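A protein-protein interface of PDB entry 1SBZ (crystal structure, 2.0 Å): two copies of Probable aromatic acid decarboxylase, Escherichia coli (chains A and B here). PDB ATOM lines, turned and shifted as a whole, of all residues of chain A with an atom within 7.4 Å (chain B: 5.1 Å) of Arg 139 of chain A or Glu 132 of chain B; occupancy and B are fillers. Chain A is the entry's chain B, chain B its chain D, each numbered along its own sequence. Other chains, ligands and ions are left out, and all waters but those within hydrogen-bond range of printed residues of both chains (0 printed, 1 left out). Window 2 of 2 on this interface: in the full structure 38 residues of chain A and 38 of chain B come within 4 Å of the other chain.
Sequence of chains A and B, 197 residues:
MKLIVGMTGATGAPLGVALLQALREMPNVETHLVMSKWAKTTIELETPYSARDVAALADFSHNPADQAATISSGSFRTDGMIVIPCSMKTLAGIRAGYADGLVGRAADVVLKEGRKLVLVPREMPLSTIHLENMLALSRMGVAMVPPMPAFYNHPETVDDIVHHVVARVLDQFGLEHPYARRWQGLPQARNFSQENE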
ATOM      1  N   LEU A 131     -28.235  23.273  14.316  1.00  0.00           N
ATOM      2  CA  LEU A 131     -27.555  23.652  13.074  1.00  0.00           C
ATOM      3  C   LEU A 131     -26.211  22.917  12.900  1.00  0.00           C
ATOM      4  O   LEU A 131     -25.872  22.499  11.792  1.00  0.00           O
ATOM      5  CB  LEU A 131     -27.432  25.178  12.961  1.00  0.00           C
ATOM      6  CG  LEU A 131     -28.768  25.922  12.781  1.00  0.00           C
ATOM      7  CD1 LEU A 131     -28.658  27.410  13.161  1.00  0.00           C
ATOM      8  CD2 LEU A 131     -29.274  25.780  11.352  1.00  0.00           C
ATOM      9  N   GLU A 132     -25.493  22.723  14.007  1.00  0.00           N
ATOM     10  CA  GLU A 132     -24.279  21.898  14.066  1.00  0.00           C
ATOM     11  C   GLU A 132     -24.529  20.478  13.573  1.00  0.00           C
ATOM     12  O   GLU A 132     -23.729  19.910  12.828  1.00  0.00           O
ATOM     13  CB  GLU A 132     -23.813  21.764  15.531  1.00  0.00           C
ATOM     14  CG  GLU A 132     -22.801  22.772  16.019  1.00  0.00           C
ATOM     15  CD  GLU A 132     -22.370  22.516  17.467  1.00  0.00           C
ATOM     16  OE1 GLU A 132     -21.276  22.986  17.831  1.00  0.00           O
ATOM     17  OE2 GLU A 132     -23.115  21.860  18.247  1.00  0.00           O
ATOM     18  N   ASN A 133     -25.628  19.893  14.042  1.00  0.00           N
ATOM     19  CA  ASN A 133     -25.965  18.514  13.733  1.00  0.00           C
ATOM     20  C   ASN A 133     -26.375  18.374  12.276  1.00  0.00           C
ATOM     21  O   ASN A 133     -25.954  17.441  11.588  1.00  0.00           O
ATOM     22  CB  ASN A 133     -27.072  18.005  14.667  1.00  0.00           C
ATOM     23  CG  ASN A 133     -26.599  17.819  16.106  1.00  0.00           C
ATOM     24  OD1 ASN A 133     -27.411  17.773  17.044  1.00  0.00           O
ATOM     25  ND2 ASN A 133     -25.304  17.700  16.288  1.00  0.00           N
ATOM     26  N   MET A 134     -27.201  19.317  11.824  1.00  0.00           N
ATOM     27  CA  MET A 134     -27.653  19.391  10.434  1.00  0.00           C
ATOM     28  C   MET A 134     -26.488  19.588   9.481  1.00  0.00           C
ATOM     29  O   MET A 134     -26.398  18.899   8.467  1.00  0.00           O
ATOM     30  CB  MET A 134     -28.670  20.520  10.268  1.00  0.00           C
ATOM     31  CG  MET A 134     -30.028  20.191  10.891  1.00  0.00           C
ATOM     32  SD  MET A 134     -31.208  21.728  11.098  1.00  0.00           S
ATOM     33  CE  MET A 134     -31.574  22.081   9.263  1.00  0.00           C
ATOM     34  N   LEU A 135     -25.599  20.524   9.806  1.00  0.00           N
ATOM     35  CA  LEU A 135     -24.405  20.769   8.990  1.00  0.00           C
ATOM     36  C   LEU A 135     -23.508  19.529   8.864  1.00  0.00           C
ATOM     37  O   LEU A 135     -23.104  19.165   7.757  1.00  0.00           O
ATOM     38  CB  LEU A 135     -23.596  21.965   9.519  1.00  0.00           C
ATOM     39  CG  LEU A 135     -22.252  22.213   8.817  1.00  0.00           C
ATOM     40  CD1 LEU A 135     -22.416  22.484   7.294  1.00  0.00           C
ATOM     41  CD2 LEU A 135     -21.469  23.339   9.478  1.00  0.00           C
ATOM     42  N   ALA A 136     -23.196  18.882   9.988  1.00  0.00           N
ATOM     43  CA  ALA A 136     -22.322  17.702   9.963  1.00  0.00           C
ATOM     44  C   ALA A 136     -22.856  16.590   9.039  1.00  0.00           C
ATOM     45  O   ALA A 136     -22.088  15.984   8.284  1.00  0.00           O
ATOM     46  CB  ALA A 136     -22.094  17.162  11.385  1.00  0.00           C
ATOM     47  N   LEU A 137     -24.162  16.330   9.115  1.00  0.00           N
ATOM     48  CA  LEU A 137     -24.826  15.350   8.234  1.00  0.00           C
ATOM     49  C   LEU A 137     -24.936  15.814   6.774  1.00  0.00           C
ATOM     50  O   LEU A 137     -24.802  15.000   5.867  1.00  0.00           O
ATOM     51  CB  LEU A 137     -26.207  14.950   8.774  1.00  0.00           C
ATOM     52  CG  LEU A 137     -26.281  14.157  10.089  1.00  0.00           C
ATOM     53  CD1 LEU A 137     -27.737  13.976  10.526  1.00  0.00           C
ATOM     54  CD2 LEU A 137     -25.586  12.807   9.962  1.00  0.00           C
ATOM     55  N   SER A 138     -25.191  17.105   6.550  1.00  0.00           N
ATOM     56  CA  SER A 138     -25.131  17.660   5.188  1.00  0.00           C
ATOM     57  C   SER A 138     -23.762  17.424   4.515  1.00  0.00           C
ATOM     58  O   SER A 138     -23.709  17.023   3.352  1.00  0.00           O
ATOM     59  CB  SER A 138     -25.501  19.137   5.176  1.00  0.00           C
ATOM     60  OG  SER A 138     -25.409  19.657   3.859  1.00  0.00           O
ATOM     61  N   ARG A 139     -22.666  17.646   5.252  1.00  0.00           N
ATOM     62  CA  ARG A 139     -21.302  17.383   4.745  1.00  0.00           C
ATOM     63  C   ARG A 139     -21.099  15.919   4.299  1.00  0.00           C
ATOM     64  O   ARG A 139     -20.246  15.627   3.458  1.00  0.00           O
ATOM     65  CB  ARG A 139     -20.244  17.745   5.796  1.00  0.00           C
ATOM     66  CG  ARG A 139     -20.138  19.227   6.121  1.00  0.00           C
ATOM     67  CD  ARG A 139     -18.883  19.644   6.910  1.00  0.00           C
ATOM     68  NE  ARG A 139     -18.675  21.083   6.742  1.00  0.00           N
ATOM     69  CZ  ARG A 139     -18.510  21.980   7.704  1.00  0.00           C
ATOM     70  NH1 ARG A 139     -18.465  21.627   8.984  1.00  0.00           N
ATOM     71  NH2 ARG A 139     -18.357  23.255   7.369  1.00  0.00           N
ATOM     72  N   MET A 140     -21.884  15.009   4.865  1.00  0.00           N
ATOM     73  CA  MET A 140     -21.864  13.594   4.482  1.00  0.00           C
ATOM     74  C   MET A 140     -22.835  13.264   3.353  1.00  0.00           C
ATOM     75  O   MET A 140     -22.995  12.096   2.990  1.00  0.00           O
ATOM     76  CB  MET A 140     -22.224  12.718   5.685  1.00  0.00           C
ATOM     77  CG  MET A 140     -21.267  12.806   6.847  1.00  0.00           C
ATOM     78  SD  MET A 140     -21.924  11.775   8.376  1.00  0.00           S
ATOM     79  CE  MET A 140     -22.222  10.043   7.514  1.00  0.00           C
ATOM     80  N   GLY A 141     -23.522  14.273   2.824  1.00  0.00           N
ATOM     81  CA  GLY A 141     -24.413  14.052   1.703  1.00  0.00           C
ATOM     82  C   GLY A 141     -25.844  13.736   2.098  1.00  0.00           C
ATOM     83  O   GLY A 141     -26.610  13.269   1.270  1.00  0.00           O
ATOM     84  N   VAL A 142     -26.205  13.981   3.358  1.00  0.00           N
ATOM     85  CA  VAL A 142     -27.593  13.810   3.800  1.00  0.00           C
ATOM     86  C   VAL A 142     -28.426  15.004   3.321  1.00  0.00           C
ATOM     87  O   VAL A 142     -28.075  16.154   3.579  1.00  0.00           O
ATOM     88  CB  VAL A 142     -27.709  13.677   5.336  1.00  0.00           C
ATOM     89  CG1 VAL A 142     -29.180  13.599   5.786  1.00  0.00           C
ATOM     90  CG2 VAL A 142     -26.904  12.485   5.841  1.00  0.00           C
ATOM     91  N   ARG B  95     -23.403  36.918   6.933  1.00  0.00           N
ATOM     92  CA  ARG B  95     -22.372  36.042   7.512  1.00  0.00           C
ATOM     93  C   ARG B  95     -20.960  36.453   7.092  1.00  0.00           C
ATOM     94  O   ARG B  95     -20.050  36.455   7.913  1.00  0.00           O
ATOM     95  CB  ARG B  95     -22.636  34.578   7.140  1.00  0.00           C
ATOM     96  CG  ARG B  95     -21.728  33.561   7.855  1.00  0.00           C
ATOM     97  CD  ARG B  95     -20.398  33.280   7.139  1.00  0.00           C
ATOM     98  NE  ARG B  95     -19.464  32.523   7.978  1.00  0.00           N
ATOM     99  CZ  ARG B  95     -18.736  33.043   8.967  1.00  0.00           C
ATOM    100  NH1 ARG B  95     -18.827  34.339   9.271  1.00  0.00           N
ATOM    101  NH2 ARG B  95     -17.917  32.263   9.666  1.00  0.00           N
ATOM    102  N   SER B 127     -28.610  23.457   1.650  1.00  0.00           N
ATOM    103  CA  SER B 127     -27.346  22.845   1.271  1.00  0.00           C
ATOM    104  C   SER B 127     -26.323  23.058   2.378  1.00  0.00           C
ATOM    105  O   SER B 127     -26.606  23.714   3.382  1.00  0.00           O
ATOM    106  CB  SER B 127     -26.840  23.452  -0.039  1.00  0.00           C
ATOM    107  OG  SER B 127     -26.346  24.762   0.190  1.00  0.00           O
ATOM    108  N   THR B 128     -25.127  22.513   2.185  1.00  0.00           N
ATOM    109  CA  THR B 128     -24.029  22.689   3.135  1.00  0.00           C
ATOM    110  C   THR B 128     -23.672  24.158   3.342  1.00  0.00           C
ATOM    111  O   THR B 128     -23.391  24.574   4.464  1.00  0.00           O
ATOM    112  CB  THR B 128     -22.789  21.871   2.683  1.00  0.00           C
ATOM    113  OG1 THR B 128     -23.117  20.482   2.714  1.00  0.00           O
ATOM    114  CG2 THR B 128     -21.652  21.958   3.712  1.00  0.00           C
ATOM    115  N   ILE B 129     -23.695  24.941   2.271  1.00  0.00           N
ATOM    116  CA  ILE B 129     -23.383  26.371   2.371  1.00  0.00           C
ATOM    117  C   ILE B 129     -24.435  27.091   3.216  1.00  0.00           C
ATOM    118  O   ILE B 129     -24.086  27.840   4.117  1.00  0.00           O
ATOM    119  CB  ILE B 129     -23.263  27.040   0.977  1.00  0.00           C
ATOM    120  CG1 ILE B 129     -22.152  26.391   0.158  1.00  0.00           C
ATOM    121  CG2 ILE B 129     -22.989  28.565   1.140  1.00  0.00           C
ATOM    122  CD1 ILE B 129     -22.191  26.755  -1.342  1.00  0.00           C
ATOM    123  N   HIS B 130     -25.712  26.858   2.922  1.00  0.00           N
ATOM    124  CA  HIS B 130     -26.796  27.454   3.703  1.00  0.00           C
ATOM    125  C   HIS B 130     -26.593  27.143   5.186  1.00  0.00           C
ATOM    126  O   HIS B 130     -26.625  28.034   6.018  1.00  0.00           O
ATOM    127  CB  HIS B 130     -28.163  26.933   3.234  1.00  0.00           C
ATOM    128  CG  HIS B 130     -28.422  27.130   1.768  1.00  0.00           C
ATOM    129  ND1 HIS B 130     -29.244  26.298   1.040  1.00  0.00           N
ATOM    130  CD2 HIS B 130     -27.976  28.073   0.901  1.00  0.00           C
ATOM    131  CE1 HIS B 130     -29.288  26.712  -0.217  1.00  0.00           C
ATOM    132  NE2 HIS B 130     -28.530  27.792  -0.327  1.00  0.00           N
ATOM    133  N   LEU B 131     -26.354  25.867   5.494  1.00  0.00           N
ATOM    134  CA  LEU B 131     -26.190  25.428   6.869  1.00  0.00           C
ATOM    135  C   LEU B 131     -24.941  26.012   7.570  1.00  0.00           C
ATOM    136  O   LEU B 131     -25.001  26.342   8.757  1.00  0.00           O
ATOM    137  CB  LEU B 131     -26.268  23.891   6.942  1.00  0.00           C
ATOM    138  CG  LEU B 131     -27.671  23.377   6.562  1.00  0.00           C
ATOM    139  CD1 LEU B 131     -27.674  21.895   6.204  1.00  0.00           C
ATOM    140  CD2 LEU B 131     -28.663  23.672   7.694  1.00  0.00           C
ATOM    141  N   GLU B 132     -23.833  26.137   6.835  1.00  0.00           N
ATOM    142  CA  GLU B 132     -22.601  26.750   7.351  1.00  0.00           C
ATOM    143  C   GLU B 132     -22.849  28.186   7.756  1.00  0.00           C
ATOM    144  O   GLU B 132     -22.458  28.605   8.840  1.00  0.00           O
ATOM    145  CB  GLU B 132     -21.512  26.796   6.278  1.00  0.00           C
ATOM    146  CG  GLU B 132     -20.641  25.572   6.141  1.00  0.00           C
ATOM    147  CD  GLU B 132     -19.646  25.716   4.995  1.00  0.00           C
ATOM    148  OE1 GLU B 132     -18.578  25.069   5.062  1.00  0.00           O
ATOM    149  OE2 GLU B 132     -19.937  26.468   4.023  1.00  0.00           O
ATOM    150  N   ASN B 133     -23.491  28.938   6.862  1.00  0.00           N
ATOM    151  CA  ASN B 133     -23.797  30.345   7.103  1.00  0.00           C
ATOM    152  C   ASN B 133     -24.757  30.515   8.274  1.00  0.00           C
ATOM    153  O   ASN B 133     -24.557  31.391   9.117  1.00  0.00           O
ATOM    154  CB  ASN B 133     -24.355  31.016   5.841  1.00  0.00           C
ATOM    155  CG  ASN B 133     -23.339  31.073   4.686  1.00  0.00           C
ATOM    156  OD1 ASN B 133     -23.719  31.228   3.518  1.00  0.00           O
ATOM    157  ND2 ASN B 133     -22.058  30.960   5.007  1.00  0.00           N
ATOM    158  N   MET B 134     -25.787  29.671   8.333  1.00  0.00           N
ATOM    159  CA  MET B 134     -26.731  29.698   9.451  1.00  0.00           C
ATOM    160  C   MET B 134     -26.061  29.407  10.793  1.00  0.00           C
ATOM    161  O   MET B 134     -26.362  30.051  11.799  1.00  0.00           O
ATOM    162  CB  MET B 134     -27.867  28.708   9.218  1.00  0.00           C
ATOM    163  CG  MET B 134     -28.838  29.194   8.161  1.00  0.00           C
ATOM    164  SD  MET B 134     -30.142  27.842   7.629  1.00  0.00           S
ATOM    165  CE  MET B 134     -31.233  27.864   9.071  1.00  0.00           C
ATOM    166  N   LEU B 135     -25.167  28.425  10.806  1.00  0.00           N
ATOM    167  CA  LEU B 135     -24.457  28.068  12.031  1.00  0.00           C
ATOM    168  C   LEU B 135     -23.512  29.192  12.494  1.00  0.00           C
ATOM    169  O   LEU B 135     -23.474  29.533  13.670  1.00  0.00           O
ATOM    170  CB  LEU B 135     -23.697  26.738  11.856  1.00  0.00           C
ATOM    171  CG  LEU B 135     -22.830  26.265  13.037  1.00  0.00           C
ATOM    172  CD1 LEU B 135     -23.642  26.034  14.316  1.00  0.00           C
ATOM    173  CD2 LEU B 135     -22.060  24.996  12.660  1.00  0.00           C
ATOM    174  N   ALA B 136     -22.749  29.756  11.566  1.00  0.00           N
ATOM    175  CA  ALA B 136     -21.792  30.805  11.914  1.00  0.00           C
ATOM    176  C   ALA B 136     -22.489  31.949  12.657  1.00  0.00           C
ATOM    177  O   ALA B 136     -22.006  32.410  13.685  1.00  0.00           O
ATOM    178  CB  ALA B 136     -21.102  31.320  10.662  1.00  0.00           C
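The backbone NH of Ile 129 of chain B lies close to the side-chain hydroxyl of Ser 127 of chain B. A ring nitrogen (ND1) of His 130 of chain B lies within hydrogen-bond range of the backbone NH (N) of Ser 127 of chain B, 3.0 Å away.
NH2 of Arg 139 of chain A is in salt-bridge range of OE1 of Glu 132 of chain B (2.9 Å). The side-chain hydroxyl (OG1) of Thr 128 of chain B is in hydrogen-bond range of the side-chain hydroxyl (OG) of Ser 138 of chain A (2.7 Å).
Leu 131 of chain A touches Met 134 of chain B, and with the chains exchanged Met 134 of chain A touches Leu 131 of chain B. Glu 132 of chain A touches Leu 135 of chain B, and with the chains exchanged Leu 135 of chain A touches Glu 132 of chain B. Leu 135 of chain A touches its own counterpart, Leu 135 of chain B. 6 positions are printed for both chains. Of the 11 pairs that touch across the chains among the printed residues, 5 have their exchanged pair printed and touching as well.
Among the printed residues, pairs that only touch across the chains: Leu 135 of chain A with Leu 135 of chain B (3.6 Å), Leu 135 of chain A with Thr 128 of chain B (3.7 Å), Leu 131 of chain A with Met 134 of chain B (3.7 Å), Ser 138 of chain A with Leu 131 of chain B (3.7 Å), Met 134 of chain A with Leu 131 of chain B (3.7 Å), Leu 135 of chain A with Glu 132 of chain B (3.7 Å), Glu 132 of chain A with Leu 135 of chain B (3.8 Å), Ser 138 of chain A with Ser 127 of chain B (3.8 Å) and Arg 139 of chain A with Thr 128 of chain B (3.8 Å).
Glu 132 of chain B touches just these residues of chain A: Leu 135 (3.7 Å) and Arg 139 (2.9 Å). Printed residues of chain B within 4 Å of Met 134 of chain A: Leu 131 (3.7 Å). Printed residues of chain A within 4 Å of Thr 128 of chain B: Leu 135 (3.7 Å), Ser 138 (2.7 Å) and Arg 139 (3.8 Å). Ala 136 of chain A touches none of the printed residues of chain B. Ala 136 of chain B touches none of the printed residues of chain A. The nearest printed residue of chain A that does not touch Leu 131 of chain B is Leu 135 of chain A (4.1 Å).
Of the 12 printed residues of chain A, 6 touch a printed residue of chain B. Hydrophobic or aromatic side chains of chain A that line the printed part of chain B: Leu 131, Met 134 and Leu 135. Along chain A the printed residues that touch a printed residue of chain B span positions 131 to 139. Of the 11 printed residues of chain B, 6 touch a printed residue of chain A. Hydrophobic or aromatic side chains of chain B within 4 Å of the printed part of chain A: Leu 131, Met 134 and Leu 135. Along chain B the printed residues that touch a printed residue of chain A span positions 127 to 135. Among the printed residues, Asp or Glu carboxylates within 4 Å of a Lys or Arg side-chain nitrogen of the other chain: Arg 139 of chain A with Glu 132 of chain B.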
